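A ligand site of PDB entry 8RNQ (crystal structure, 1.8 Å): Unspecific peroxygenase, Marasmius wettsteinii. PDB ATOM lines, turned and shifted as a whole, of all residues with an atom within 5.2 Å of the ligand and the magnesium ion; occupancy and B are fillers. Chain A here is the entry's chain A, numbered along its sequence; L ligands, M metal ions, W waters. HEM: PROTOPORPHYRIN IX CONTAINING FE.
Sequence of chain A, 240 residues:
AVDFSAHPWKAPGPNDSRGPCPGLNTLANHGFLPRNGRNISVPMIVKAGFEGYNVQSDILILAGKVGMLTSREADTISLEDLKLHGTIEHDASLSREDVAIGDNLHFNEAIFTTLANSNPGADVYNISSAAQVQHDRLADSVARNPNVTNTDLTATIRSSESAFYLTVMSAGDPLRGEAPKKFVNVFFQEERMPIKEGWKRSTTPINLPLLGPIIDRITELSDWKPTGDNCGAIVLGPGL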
ATOM      1  N   PRO A  20     -25.045 -30.465 -17.115  1.00  0.00           N
ATOM      2  CA  PRO A  20     -24.155 -29.363 -17.478  1.00  0.00           C
ATOM      3  C   PRO A  20     -24.574 -27.980 -17.001  1.00  0.00           C
ATOM      4  O   PRO A  20     -23.873 -27.015 -17.240  1.00  0.00           O
ATOM      5  CB  PRO A  20     -24.210 -29.414 -19.019  1.00  0.00           C
ATOM      6  CG  PRO A  20     -25.598 -29.875 -19.343  1.00  0.00           C
ATOM      7  CD  PRO A  20     -25.982 -30.813 -18.202  1.00  0.00           C
ATOM      8  N   CYS A  21     -25.735 -27.921 -16.327  1.00  0.00           N
ATOM      9  CA  CYS A  21     -26.339 -26.653 -15.929  1.00  0.00           C
ATOM     10  C   CYS A  21     -26.127 -26.416 -14.439  1.00  0.00           C
ATOM     11  O   CYS A  21     -26.726 -27.097 -13.618  1.00  0.00           O
ATOM     12  CB  CYS A  21     -27.812 -26.615 -16.228  1.00  0.00           C
ATOM     13  SG  CYS A  21     -28.629 -25.114 -15.614  1.00  0.00           S
ATOM     14  N   PRO A  22     -25.344 -25.399 -14.062  1.00  0.00           N
ATOM     15  CA  PRO A  22     -25.167 -25.065 -12.638  1.00  0.00           C
ATOM     16  C   PRO A  22     -26.449 -24.554 -11.975  1.00  0.00           C
ATOM     17  O   PRO A  22     -26.632 -24.696 -10.764  1.00  0.00           O
ATOM     18  CB  PRO A  22     -24.102 -23.976 -12.644  1.00  0.00           C
ATOM     19  CG  PRO A  22     -24.223 -23.337 -14.044  1.00  0.00           C
ATOM     20  CD  PRO A  22     -24.607 -24.487 -14.933  1.00  0.00           C
ATOM     21  N   GLY A  23     -27.366 -23.992 -12.776  1.00  0.00           N
ATOM     22  CA  GLY A  23     -28.592 -23.472 -12.203  1.00  0.00           C
ATOM     23  C   GLY A  23     -29.472 -24.590 -11.654  1.00  0.00           C
ATOM     24  O   GLY A  23     -29.986 -24.539 -10.539  1.00  0.00           O
ATOM     25  N   LEU A  24     -29.691 -25.611 -12.487  1.00  0.00           N
ATOM     26  CA  LEU A  24     -30.497 -26.741 -12.099  1.00  0.00           C
ATOM     27  C   LEU A  24     -29.743 -27.610 -11.080  1.00  0.00           C
ATOM     28  O   LEU A  24     -30.372 -28.154 -10.172  1.00  0.00           O
ATOM     29  CB  LEU A  24     -30.888 -27.547 -13.341  1.00  0.00           C
ATOM     30  CG  LEU A  24     -31.781 -26.788 -14.336  1.00  0.00           C
ATOM     31  CD1 LEU A  24     -32.136 -27.681 -15.490  1.00  0.00           C
ATOM     32  CD2 LEU A  24     -33.056 -26.240 -13.676  1.00  0.00           C
ATOM     33  N   LEU A  27     -30.165 -26.039  -7.657  1.00  0.00           N
ATOM     34  CA  LEU A  27     -31.488 -26.268  -7.114  1.00  0.00           C
ATOM     35  C   LEU A  27     -31.605 -27.684  -6.545  1.00  0.00           C
ATOM     36  O   LEU A  27     -32.188 -27.884  -5.471  1.00  0.00           O
ATOM     37  CB  LEU A  27     -32.532 -25.972  -8.200  1.00  0.00           C
ATOM     38  CG  LEU A  27     -32.694 -24.507  -8.586  1.00  0.00           C
ATOM     39  CD1 LEU A  27     -33.601 -24.383  -9.802  1.00  0.00           C
ATOM     40  CD2 LEU A  27     -33.257 -23.686  -7.438  1.00  0.00           C
ATOM     41  N   ILE A  45     -39.445 -27.729 -12.546  1.00  0.00           N
ATOM     42  CA  ILE A  45     -38.436 -26.730 -12.846  1.00  0.00           C
ATOM     43  C   ILE A  45     -39.000 -25.314 -12.624  1.00  0.00           C
ATOM     44  O   ILE A  45     -38.321 -24.452 -12.076  1.00  0.00           O
ATOM     45  CB  ILE A  45     -37.892 -26.917 -14.286  1.00  0.00           C
ATOM     46  CG1 ILE A  45     -37.063 -28.193 -14.387  1.00  0.00           C
ATOM     47  CG2 ILE A  45     -37.090 -25.721 -14.685  1.00  0.00           C
ATOM     48  CD1 ILE A  45     -36.749 -28.664 -15.806  1.00  0.00           C
ATOM     49  N   TYR A  53     -34.800 -18.840  -7.001  1.00  0.00           N
ATOM     50  CA  TYR A  53     -34.074 -17.767  -7.653  1.00  0.00           C
ATOM     51  C   TYR A  53     -34.963 -16.572  -8.043  1.00  0.00           C
ATOM     52  O   TYR A  53     -34.419 -15.528  -8.450  1.00  0.00           O
ATOM     53  CB  TYR A  53     -33.438 -18.259  -8.973  1.00  0.00           C
ATOM     54  CG  TYR A  53     -32.441 -19.389  -8.902  1.00  0.00           C
ATOM     55  CD1 TYR A  53     -31.499 -19.487  -7.891  1.00  0.00           C
ATOM     56  CD2 TYR A  53     -32.373 -20.335  -9.908  1.00  0.00           C
ATOM     57  CE1 TYR A  53     -30.566 -20.501  -7.857  1.00  0.00           C
ATOM     58  CE2 TYR A  53     -31.458 -21.380  -9.883  1.00  0.00           C
ATOM     59  CZ  TYR A  53     -30.508 -21.441  -8.876  1.00  0.00           C
ATOM     60  OH  TYR A  53     -29.581 -22.459  -8.813  1.00  0.00           O
ATOM     61  N   VAL A  55     -36.801 -16.759 -10.619  1.00  0.00           N
ATOM     62  CA  VAL A  55     -36.913 -16.808 -12.079  1.00  0.00           C
ATOM     63  C   VAL A  55     -38.325 -17.234 -12.455  1.00  0.00           C
ATOM     64  O   VAL A  55     -38.886 -18.159 -11.900  1.00  0.00           O
ATOM     65  CB  VAL A  55     -35.833 -17.712 -12.690  1.00  0.00           C
ATOM     66  CG1 VAL A  55     -36.035 -17.889 -14.190  1.00  0.00           C
ATOM     67  CG2 VAL A  55     -34.446 -17.216 -12.414  1.00  0.00           C
ATOM     68  N   ILE A  59     -39.383 -17.926 -19.074  1.00  0.00           N
ATOM     69  CA  ILE A  59     -38.123 -18.476 -19.603  1.00  0.00           C
ATOM     70  C   ILE A  59     -38.001 -19.958 -19.250  1.00  0.00           C
ATOM     71  O   ILE A  59     -37.430 -20.738 -20.017  1.00  0.00           O
ATOM     72  CB  ILE A  59     -36.895 -17.665 -19.148  1.00  0.00           C
ATOM     73  CG1 ILE A  59     -35.638 -18.220 -19.813  1.00  0.00           C
ATOM     74  CG2 ILE A  59     -36.798 -17.636 -17.643  1.00  0.00           C
ATOM     75  CD1 ILE A  59     -34.423 -17.342 -19.734  1.00  0.00           C
ATOM     76  N   LEU A  60     -38.532 -20.381 -18.085  1.00  0.00           N
ATOM     77  CA  LEU A  60     -38.386 -21.758 -17.627  1.00  0.00           C
ATOM     78  C   LEU A  60     -39.276 -22.718 -18.392  1.00  0.00           C
ATOM     79  O   LEU A  60     -38.862 -23.862 -18.596  1.00  0.00           O
ATOM     80  CB  LEU A  60     -38.637 -21.836 -16.121  1.00  0.00           C
ATOM     81  CG  LEU A  60     -37.606 -21.090 -15.275  1.00  0.00           C
ATOM     82  CD1 LEU A  60     -37.930 -21.189 -13.798  1.00  0.00           C
ATOM     83  CD2 LEU A  60     -36.173 -21.606 -15.512  1.00  0.00           C
ATOM     84  N   ALA A  63     -37.356 -22.891 -22.031  1.00  0.00           N
ATOM     85  CA  ALA A  63     -36.133 -23.698 -21.912  1.00  0.00           C
ATOM     86  C   ALA A  63     -36.435 -25.128 -21.469  1.00  0.00           C
ATOM     87  O   ALA A  63     -35.853 -26.070 -21.978  1.00  0.00           O
ATOM     88  CB  ALA A  63     -35.157 -23.062 -20.939  1.00  0.00           C
ATOM     89  N   GLY A  64     -37.362 -25.272 -20.505  1.00  0.00           N
ATOM     90  CA  GLY A  64     -37.699 -26.569 -19.946  1.00  0.00           C
ATOM     91  C   GLY A  64     -38.217 -27.541 -21.002  1.00  0.00           C
ATOM     92  O   GLY A  64     -37.863 -28.722 -21.018  1.00  0.00           O
ATOM     93  N   GLY A  67     -35.529 -28.722 -23.101  1.00  0.00           N
ATOM     94  CA  GLY A  67     -34.766 -29.696 -22.344  1.00  0.00           C
ATOM     95  C   GLY A  67     -35.425 -31.074 -22.271  1.00  0.00           C
ATOM     96  O   GLY A  67     -34.747 -32.086 -22.222  1.00  0.00           O
ATOM     97  N   LEU A  82     -29.471 -33.624 -19.962  1.00  0.00           N
ATOM     98  CA  LEU A  82     -29.319 -32.321 -20.593  1.00  0.00           C
ATOM     99  C   LEU A  82     -27.944 -32.149 -21.267  1.00  0.00           C
ATOM    100  O   LEU A  82     -27.718 -31.151 -21.958  1.00  0.00           O
ATOM    101  CB  LEU A  82     -29.522 -31.230 -19.543  1.00  0.00           C
ATOM    102  CG  LEU A  82     -30.948 -31.099 -19.010  1.00  0.00           C
ATOM    103  CD1 LEU A  82     -30.997 -30.094 -17.887  1.00  0.00           C
ATOM    104  CD2 LEU A  82     -31.934 -30.719 -20.112  1.00  0.00           C
ATOM    105  N   ILE A  88     -29.695 -28.235 -26.211  1.00  0.00           N
ATOM    106  CA  ILE A  88     -29.246 -26.997 -25.606  1.00  0.00           C
ATOM    107  C   ILE A  88     -27.710 -26.977 -25.461  1.00  0.00           C
ATOM    108  O   ILE A  88     -27.065 -25.961 -25.704  1.00  0.00           O
ATOM    109  CB  ILE A  88     -29.941 -26.777 -24.246  1.00  0.00           C
ATOM    110  CG1 ILE A  88     -31.457 -26.555 -24.403  1.00  0.00           C
ATOM    111  CG2 ILE A  88     -29.318 -25.608 -23.509  1.00  0.00           C
ATOM    112  CD1 ILE A  88     -32.222 -26.553 -23.091  1.00  0.00           C
ATOM    113  N   GLU A  89     -27.121 -28.092 -25.021  1.00  0.00           N
ATOM    114  CA  GLU A  89     -25.685 -28.148 -24.723  1.00  0.00           C
ATOM    115  C   GLU A  89     -24.874 -27.769 -25.967  1.00  0.00           C
ATOM    116  O   GLU A  89     -25.192 -28.194 -27.074  1.00  0.00           O
ATOM    117  CB  GLU A  89     -25.298 -29.517 -24.170  1.00  0.00           C
ATOM    118  CG  GLU A  89     -23.918 -29.538 -23.538  1.00  0.00           C
ATOM    119  CD  GLU A  89     -22.756 -29.548 -24.525  1.00  0.00           C
ATOM    120  OE1 GLU A  89     -22.897 -30.261 -25.522  1.00  0.00           O
ATOM    121  OE2 GLU A  89     -21.755 -28.844 -24.260  1.00  0.00           O
ATOM    122  N   HIS A  90     -23.900 -26.887 -25.765  1.00  0.00           N
ATOM    123  CA  HIS A  90     -23.173 -26.266 -26.857  1.00  0.00           C
ATOM    124  C   HIS A  90     -21.696 -26.205 -26.532  1.00  0.00           C
ATOM    125  O   HIS A  90     -21.247 -26.228 -25.381  1.00  0.00           O
ATOM    126  CB  HIS A  90     -23.736 -24.849 -27.111  1.00  0.00           C
ATOM    127  CG  HIS A  90     -23.694 -24.017 -25.880  1.00  0.00           C
ATOM    128  ND1 HIS A  90     -22.549 -23.504 -25.302  1.00  0.00           N
ATOM    129  CD2 HIS A  90     -24.729 -23.687 -25.044  1.00  0.00           C
ATOM    130  CE1 HIS A  90     -22.868 -22.923 -24.157  1.00  0.00           C
ATOM    131  NE2 HIS A  90     -24.193 -23.015 -23.977  1.00  0.00           N
ATOM    132  N   ASP A  91     -20.888 -25.968 -27.581  1.00  0.00           N
ATOM    133  CA  ASP A  91     -19.479 -25.634 -27.406  1.00  0.00           C
ATOM    134  C   ASP A  91     -19.292 -24.241 -26.805  1.00  0.00           C
ATOM    135  O   ASP A  91     -20.229 -23.429 -26.786  1.00  0.00           O
ATOM    136  CB  ASP A  91     -18.780 -25.708 -28.774  1.00  0.00           C
ATOM    137  CG  ASP A  91     -18.884 -27.070 -29.436  1.00  0.00           C
ATOM    138  OD1 ASP A  91     -18.903 -28.063 -28.689  1.00  0.00           O
ATOM    139  OD2 ASP A  91     -18.902 -27.128 -30.701  1.00  0.00           O
ATOM    140  N   SER A  93     -18.700 -23.407 -23.744  1.00  0.00           N
ATOM    141  CA  SER A  93     -19.233 -23.266 -22.392  1.00  0.00           C
ATOM    142  C   SER A  93     -18.254 -22.514 -21.494  1.00  0.00           C
ATOM    143  O   SER A  93     -17.073 -22.395 -21.764  1.00  0.00           O
ATOM    144  CB  SER A  93     -19.550 -24.642 -21.819  1.00  0.00           C
ATOM    145  OG  SER A  93     -20.628 -25.275 -22.483  1.00  0.00           O
ATOM    146  N   LEU A  94     -18.792 -21.965 -20.402  1.00  0.00           N
ATOM    147  CA  LEU A  94     -18.008 -21.172 -19.479  1.00  0.00           C
ATOM    148  C   LEU A  94     -17.205 -22.049 -18.502  1.00  0.00           C
ATOM    149  O   LEU A  94     -16.315 -21.535 -17.866  1.00  0.00           O
ATOM    150  CB  LEU A  94     -18.981 -20.282 -18.670  1.00  0.00           C
ATOM    151  CG  LEU A  94     -19.819 -19.255 -19.447  1.00  0.00           C
ATOM    152  CD1 LEU A  94     -20.997 -18.727 -18.582  1.00  0.00           C
ATOM    153  CD2 LEU A  94     -18.965 -18.129 -19.959  1.00  0.00           C
ATOM    154  N   SER A  95     -17.651 -23.282 -18.257  1.00  0.00           N
ATOM    155  CA  SER A  95     -17.155 -24.087 -17.150  1.00  0.00           C
ATOM    156  C   SER A  95     -17.017 -25.572 -17.518  1.00  0.00           C
ATOM    157  O   SER A  95     -16.652 -26.381 -16.658  1.00  0.00           O
ATOM    158  CB  SER A  95     -18.023 -23.886 -15.904  1.00  0.00           C
ATOM    159  OG  SER A  95     -19.239 -24.587 -16.019  1.00  0.00           O
ATOM    160  N   ARG A  96     -17.376 -25.943 -18.761  1.00  0.00           N
ATOM    161  CA  ARG A  96     -17.302 -27.297 -19.268  1.00  0.00           C
ATOM    162  C   ARG A  96     -16.479 -27.295 -20.556  1.00  0.00           C
ATOM    163  O   ARG A  96     -16.376 -26.268 -21.217  1.00  0.00           O
ATOM    164  CB  ARG A  96     -18.681 -27.865 -19.575  1.00  0.00           C
ATOM    165  CG  ARG A  96     -19.390 -28.568 -18.419  1.00  0.00           C
ATOM    166  CD  ARG A  96     -19.677 -27.688 -17.222  1.00  0.00           C
ATOM    167  NE  ARG A  96     -20.611 -28.329 -16.323  1.00  0.00           N
ATOM    168  CZ  ARG A  96     -20.916 -27.865 -15.121  1.00  0.00           C
ATOM    169  NH1 ARG A  96     -20.463 -26.683 -14.720  1.00  0.00           N
ATOM    170  NH2 ARG A  96     -21.700 -28.597 -14.327  1.00  0.00           N
ATOM    171  N   GLU A  97     -15.979 -28.469 -20.932  1.00  0.00           N
ATOM    172  CA  GLU A  97     -15.179 -28.603 -22.162  1.00  0.00           C
ATOM    173  C   GLU A  97     -16.118 -28.927 -23.318  1.00  0.00           C
ATOM    174  O   GLU A  97     -17.240 -29.412 -23.111  1.00  0.00           O
ATOM    175  CB  GLU A  97     -14.151 -29.734 -22.001  1.00  0.00           C
ATOM    176  CG  GLU A  97     -13.136 -29.471 -20.899  1.00  0.00           C
ATOM    177  CD  GLU A  97     -12.183 -30.633 -20.584  1.00  0.00           C
ATOM    178  OE1 GLU A  97     -12.555 -31.788 -20.797  1.00  0.00           O
ATOM    179  OE2 GLU A  97     -11.033 -30.352 -20.174  1.00  0.00           O
ATOM    180  N   ASN A 104     -18.219 -32.643 -21.523  1.00  0.00           N
ATOM    181  CA  ASN A 104     -19.163 -31.558 -21.745  1.00  0.00           C
ATOM    182  C   ASN A 104     -20.148 -31.486 -20.565  1.00  0.00           C
ATOM    183  O   ASN A 104     -21.108 -30.713 -20.640  1.00  0.00           O
ATOM    184  CB  ASN A 104     -19.929 -31.685 -23.061  1.00  0.00           C
ATOM    185  CG  ASN A 104     -20.968 -32.782 -23.093  1.00  0.00           C
ATOM    186  OD1 ASN A 104     -20.942 -33.723 -22.307  1.00  0.00           O
ATOM    187  ND2 ASN A 104     -21.912 -32.668 -24.009  1.00  0.00           N
ATOM    188  N   GLU A 161     -27.207 -17.592 -20.787  1.00  0.00           N
ATOM    189  CA  GLU A 161     -26.560 -18.239 -19.665  1.00  0.00           C
ATOM    190  C   GLU A 161     -25.735 -17.243 -18.888  1.00  0.00           C
ATOM    191  O   GLU A 161     -25.704 -17.299 -17.648  1.00  0.00           O
ATOM    192  CB  GLU A 161     -25.785 -19.467 -20.164  1.00  0.00           C
ATOM    193  CG  GLU A 161     -26.722 -20.585 -20.600  1.00  0.00           C
ATOM    194  CD  GLU A 161     -26.219 -21.675 -21.553  1.00  0.00           C
ATOM    195  OE1 GLU A 161     -25.080 -21.636 -21.948  1.00  0.00           O
ATOM    196  OE2 GLU A 161     -27.013 -22.614 -21.817  1.00  0.00           O
ATOM    197  N   PHE A 164     -28.012 -15.136 -16.943  1.00  0.00           N
ATOM    198  CA  PHE A 164     -28.475 -15.880 -15.791  1.00  0.00           C
ATOM    199  C   PHE A 164     -27.498 -15.726 -14.621  1.00  0.00           C
ATOM    200  O   PHE A 164     -27.922 -15.390 -13.515  1.00  0.00           O
ATOM    201  CB  PHE A 164     -28.720 -17.345 -16.116  1.00  0.00           C
ATOM    202  CG  PHE A 164     -30.133 -17.719 -16.453  1.00  0.00           C
ATOM    203  CD1 PHE A 164     -31.195 -17.141 -15.752  1.00  0.00           C
ATOM    204  CD2 PHE A 164     -30.410 -18.777 -17.304  1.00  0.00           C
ATOM    205  CE1 PHE A 164     -32.507 -17.515 -16.005  1.00  0.00           C
ATOM    206  CE2 PHE A 164     -31.720 -19.162 -17.547  1.00  0.00           C
ATOM    207  CZ  PHE A 164     -32.770 -18.532 -16.888  1.00  0.00           C
ATOM    208  N   TYR A 165     -26.190 -15.960 -14.822  1.00  0.00           N
ATOM    209  CA  TYR A 165     -25.334 -15.874 -13.637  1.00  0.00           C
ATOM    210  C   TYR A 165     -25.241 -14.444 -13.123  1.00  0.00           C
ATOM    211  O   TYR A 165     -25.180 -14.253 -11.901  1.00  0.00           O
ATOM    212  CB  TYR A 165     -23.975 -16.548 -13.842  1.00  0.00           C
ATOM    213  CG  TYR A 165     -22.931 -15.818 -14.630  1.00  0.00           C
ATOM    214  CD1 TYR A 165     -22.322 -14.688 -14.140  1.00  0.00           C
ATOM    215  CD2 TYR A 165     -22.516 -16.318 -15.845  1.00  0.00           C
ATOM    216  CE1 TYR A 165     -21.347 -14.026 -14.861  1.00  0.00           C
ATOM    217  CE2 TYR A 165     -21.554 -15.683 -16.593  1.00  0.00           C
ATOM    218  CZ  TYR A 165     -20.966 -14.529 -16.104  1.00  0.00           C
ATOM    219  OH  TYR A 165     -19.965 -13.889 -16.802  1.00  0.00           O
ATOM    220  N   VAL A 168     -29.121 -14.022 -11.287  1.00  0.00           N
ATOM    221  CA  VAL A 168     -29.617 -14.887 -10.223  1.00  0.00           C
ATOM    222  C   VAL A 168     -28.691 -14.781  -8.998  1.00  0.00           C
ATOM    223  O   VAL A 168     -29.130 -14.896  -7.850  1.00  0.00           O
ATOM    224  CB  VAL A 168     -29.768 -16.320 -10.771  1.00  0.00           C
ATOM    225  CG1 VAL A 168     -29.866 -17.355  -9.684  1.00  0.00           C
ATOM    226  CG2 VAL A 168     -30.956 -16.450 -11.715  1.00  0.00           C
ATOM    227  N   PHE A 187     -21.342 -20.457  -6.933  1.00  0.00           N
ATOM    228  CA  PHE A 187     -22.387 -21.021  -7.776  1.00  0.00           C
ATOM    229  C   PHE A 187     -21.810 -22.052  -8.765  1.00  0.00           C
ATOM    230  O   PHE A 187     -22.302 -23.192  -8.858  1.00  0.00           O
ATOM    231  CB  PHE A 187     -23.116 -19.848  -8.454  1.00  0.00           C
ATOM    232  CG  PHE A 187     -24.189 -20.244  -9.423  1.00  0.00           C
ATOM    233  CD1 PHE A 187     -25.375 -20.823  -9.006  1.00  0.00           C
ATOM    234  CD2 PHE A 187     -24.040 -19.967 -10.767  1.00  0.00           C
ATOM    235  CE1 PHE A 187     -26.383 -21.147  -9.919  1.00  0.00           C
ATOM    236  CE2 PHE A 187     -25.022 -20.301 -11.675  1.00  0.00           C
ATOM    237  CZ  PHE A 187     -26.201 -20.879 -11.246  1.00  0.00           C
ATOM    238  N   PHE A 188     -20.770 -21.690  -9.516  1.00  0.00           N
ATOM    239  CA  PHE A 188     -20.165 -22.576 -10.509  1.00  0.00           C
ATOM    240  C   PHE A 188     -19.323 -23.684  -9.858  1.00  0.00           C
ATOM    241  O   PHE A 188     -19.456 -24.864 -10.230  1.00  0.00           O
ATOM    242  CB  PHE A 188     -19.285 -21.759 -11.455  1.00  0.00           C
ATOM    243  CG  PHE A 188     -20.000 -21.086 -12.620  1.00  0.00           C
ATOM    244  CD1 PHE A 188     -20.238 -21.769 -13.799  1.00  0.00           C
ATOM    245  CD2 PHE A 188     -20.420 -19.774 -12.537  1.00  0.00           C
ATOM    246  CE1 PHE A 188     -20.861 -21.135 -14.866  1.00  0.00           C
ATOM    247  CE2 PHE A 188     -21.029 -19.144 -13.611  1.00  0.00           C
ATOM    248  CZ  PHE A 188     -21.247 -19.829 -14.776  1.00  0.00           C
HETATM  249  CHA HEM L   1     -26.052 -24.095 -18.908  1.00  0.00           C
HETATM  250  CHB HEM L   1     -30.291 -26.177 -19.401  1.00  0.00           C
HETATM  251  CHC HEM L   1     -32.174 -23.087 -16.186  1.00  0.00           C
HETATM  252  CHD HEM L   1     -27.819 -21.156 -15.588  1.00  0.00           C
HETATM  253  C1A HEM L   1     -27.028 -24.927 -19.259  1.00  0.00           C
HETATM  254  C2A HEM L   1     -26.837 -26.007 -20.206  1.00  0.00           C
HETATM  255  C3A HEM L   1     -28.011 -26.633 -20.311  1.00  0.00           C
HETATM  256  C4A HEM L   1     -28.955 -25.885 -19.497  1.00  0.00           C
HETATM  257  CMA HEM L   1     -28.345 -27.829 -21.143  1.00  0.00           C
HETATM  258  CAA HEM L   1     -25.504 -26.399 -20.799  1.00  0.00           C
HETATM  259  CBA HEM L   1     -25.167 -25.363 -21.894  1.00  0.00           C
HETATM  260  CGA HEM L   1     -23.689 -25.471 -22.174  1.00  0.00           C
HETATM  261  O1A HEM L   1     -23.242 -26.204 -23.055  1.00  0.00           O
HETATM  262  O2A HEM L   1     -22.908 -24.822 -21.490  1.00  0.00           O
HETATM  263  C1B HEM L   1     -31.213 -25.473 -18.598  1.00  0.00           C
HETATM  264  C2B HEM L   1     -32.582 -25.765 -18.582  1.00  0.00           C
HETATM  265  C3B HEM L   1     -33.126 -24.892 -17.660  1.00  0.00           C
HETATM  266  C4B HEM L   1     -32.029 -24.054 -17.189  1.00  0.00           C
HETATM  267  CMB HEM L   1     -33.336 -26.830 -19.301  1.00  0.00           C
HETATM  268  CAB HEM L   1     -34.533 -24.657 -17.273  1.00  0.00           C
HETATM  269  CBB HEM L   1     -35.560 -24.865 -18.028  1.00  0.00           C
HETATM  270  C1C HEM L   1     -31.152 -22.388 -15.628  1.00  0.00           C
HETATM  271  C2C HEM L   1     -31.252 -21.494 -14.512  1.00  0.00           C
HETATM  272  C3C HEM L   1     -30.046 -20.910 -14.376  1.00  0.00           C
HETATM  273  C4C HEM L   1     -29.134 -21.466 -15.376  1.00  0.00           C
HETATM  274  CMC HEM L   1     -32.591 -21.323 -13.748  1.00  0.00           C
HETATM  275  CAC HEM L   1     -29.772 -19.962 -13.304  1.00  0.00           C
HETATM  276  CBC HEM L   1     -28.723 -19.228 -13.211  1.00  0.00           C
HETATM  277  C1D HEM L   1     -26.953 -21.793 -16.496  1.00  0.00           C
HETATM  278  C2D HEM L   1     -25.577 -21.342 -16.745  1.00  0.00           C
HETATM  279  C3D HEM L   1     -25.082 -22.194 -17.685  1.00  0.00           C
HETATM  280  C4D HEM L   1     -26.190 -23.067 -17.988  1.00  0.00           C
HETATM  281  CMD HEM L   1     -24.833 -20.237 -16.053  1.00  0.00           C
HETATM  282  CAD HEM L   1     -23.673 -22.109 -18.262  1.00  0.00           C
HETATM  283  CBD HEM L   1     -22.741 -23.252 -17.865  1.00  0.00           C
HETATM  284  CGD HEM L   1     -21.438 -23.108 -18.642  1.00  0.00           C
HETATM  285  O1D HEM L   1     -21.353 -22.326 -19.645  1.00  0.00           O
HETATM  286  O2D HEM L   1     -20.439 -23.724 -18.235  1.00  0.00           O
HETATM  287  NA  HEM L   1     -28.316 -24.868 -18.893  1.00  0.00           N
HETATM  288  NB  HEM L   1     -30.875 -24.429 -17.777  1.00  0.00           N
HETATM  289  NC  HEM L   1     -29.882 -22.330 -16.074  1.00  0.00           N
HETATM  290  ND  HEM L   1     -27.354 -22.811 -17.296  1.00  0.00           N
HETATM  291 FE   HEM L   1     -29.016 -23.674 -17.419  1.00  0.00          FE
HETATM  292 MG    MG M   1     -21.243 -27.053 -23.320  1.00  0.00          MG
HETATM  293  O   HOH W   1     -22.029 -26.526 -19.326  1.00  0.00           O
HETATM  294  O   HOH W   2     -29.453 -22.327 -19.146  1.00  0.00           O
HETATM  295  O   HOH W   3     -21.508 -28.099 -21.517  1.00  0.00           O
HETATM  296  O   HOH W   4     -22.488 -20.883 -21.615  1.00  0.00           O
HETATM  297  O   HOH W   5     -19.155 -27.487 -23.556  1.00  0.00           O
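An oxygen (O2D) of the ligand lies within hydrogen-bond range of the side-chain hydroxyl (OG) of Ser 95, 2.7 Å away. An oxygen (O2D) of the ligand sits at hydrogen-bond distance from the backbone NH (N) of Ser 95 (2.8 Å). O1A of the ligand sits close to N of His 90 (2.9 Å). An iron atom (FE) of the ligand is bound by the side-chain sulfur (SG) of Cys 21, 2.3 Å away. NE2 of His 90 lies close to O2A of the ligand (3.3 Å). N of Leu 94 lies within hydrogen-bond range of O1D of the ligand, 2.7 Å away.
The magnesium ion is bound by the side-chain hydroxyl (OG) of Ser 93 (2.1 Å), the side-chain carboxylate (OE2) of Glu 89 (2.1 Å), water W3 (2.1 Å), water W5 (2.1 Å), an oxygen (O1A) of the ligand (2.2 Å) and the backbone carbonyl oxygen (O) of His 90 (2.2 Å). The magnesium ion has six donor atoms within binding distance.
Water W4 lies within hydrogen-bond range of O1D of the ligand (2.7 Å) and OE1 of Glu 161 (2.7 Å). Water W1 lies within hydrogen-bond range of the backbone carbonyl oxygen (O) of Pro 20 (2.8 Å) and an oxygen (O2A) of the ligand (2.9 Å).
Pro 20 touches the ligand (CB to CAA, 3.7 Å). CD of Pro 22 touches C3D of the ligand (3.6 Å). Gly 23 touches the ligand. Leu 24 touches the ligand (CD1 to C2B, 3.7 Å). Ile 45 touches the ligand. CD2 of Tyr 53 touches CMC of the ligand, 3.97 Å away. Leu 60 touches the ligand. CB of Ala 63 touches CBB of the ligand, at 3.4 Å. N of Gly 64 touches CBB of the ligand, 3.1 Å away. O of Leu 82 touches CMA of the ligand, 3.5 Å away. Ile 88 touches the ligand. Arg 96 touches the ligand. Glu 161 touches the ligand. CB of Phe 164 touches CBC of the ligand, 3.5 Å away. Val 168 touches the ligand. CZ of Phe 187 touches CBC of the ligand, 3.6 Å away. CZ of Phe 188 touches CMD of the ligand, at 3.8 Å. Hydrophobic or aromatic side chains within 4 Å of the ligand: Pro 20, Pro 22, Leu 24, Ile 45, Tyr 53, Leu 60, Ala 63, Leu 82, Ile 88, His 90, Leu 94, Phe 164, Val 168, Phe 187 and Phe 188. 23 residues have an atom within 4 Å of the ligand: Pro 20, Cys 21, Pro 22, Gly 23, Leu 24, Ile 45, Tyr 53, Leu 60, Ala 63, Gly 64, Leu 82, Ile 88, Glu 89, His 90, Ser 93, Leu 94, Ser 95, Arg 96, Glu 161, Phe 164, Val 168, Phe 187 and Phe 188.
Within 4 Å of the magnesium ion: Glu 89, His 90 and Ser 93.
The side-chain sulfur of Cys 21 sits close to the backbone NH of Leu 24, 3.3 Å away. OG of Ser 95 sits at hydrogen-bond distance from NH1 of Arg 96 (2.8 Å). OE1 of Glu 89 lies within hydrogen-bond range of ND2 of Asn 104 (3.0 Å). The side-chain carboxylate (OE1) of Glu 161 sits at hydrogen-bond distance from a ring nitrogen (NE2) of His 90 (2.6 Å). The side-chain sulfur (SG) of Cys 21 lies close to the backbone NH (N) of Gly 23, at 3.3 Å. The backbone carbonyl oxygen (O) of Gly 23 sits at hydrogen-bond distance from the side-chain hydroxyl (OH) of Tyr 53.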
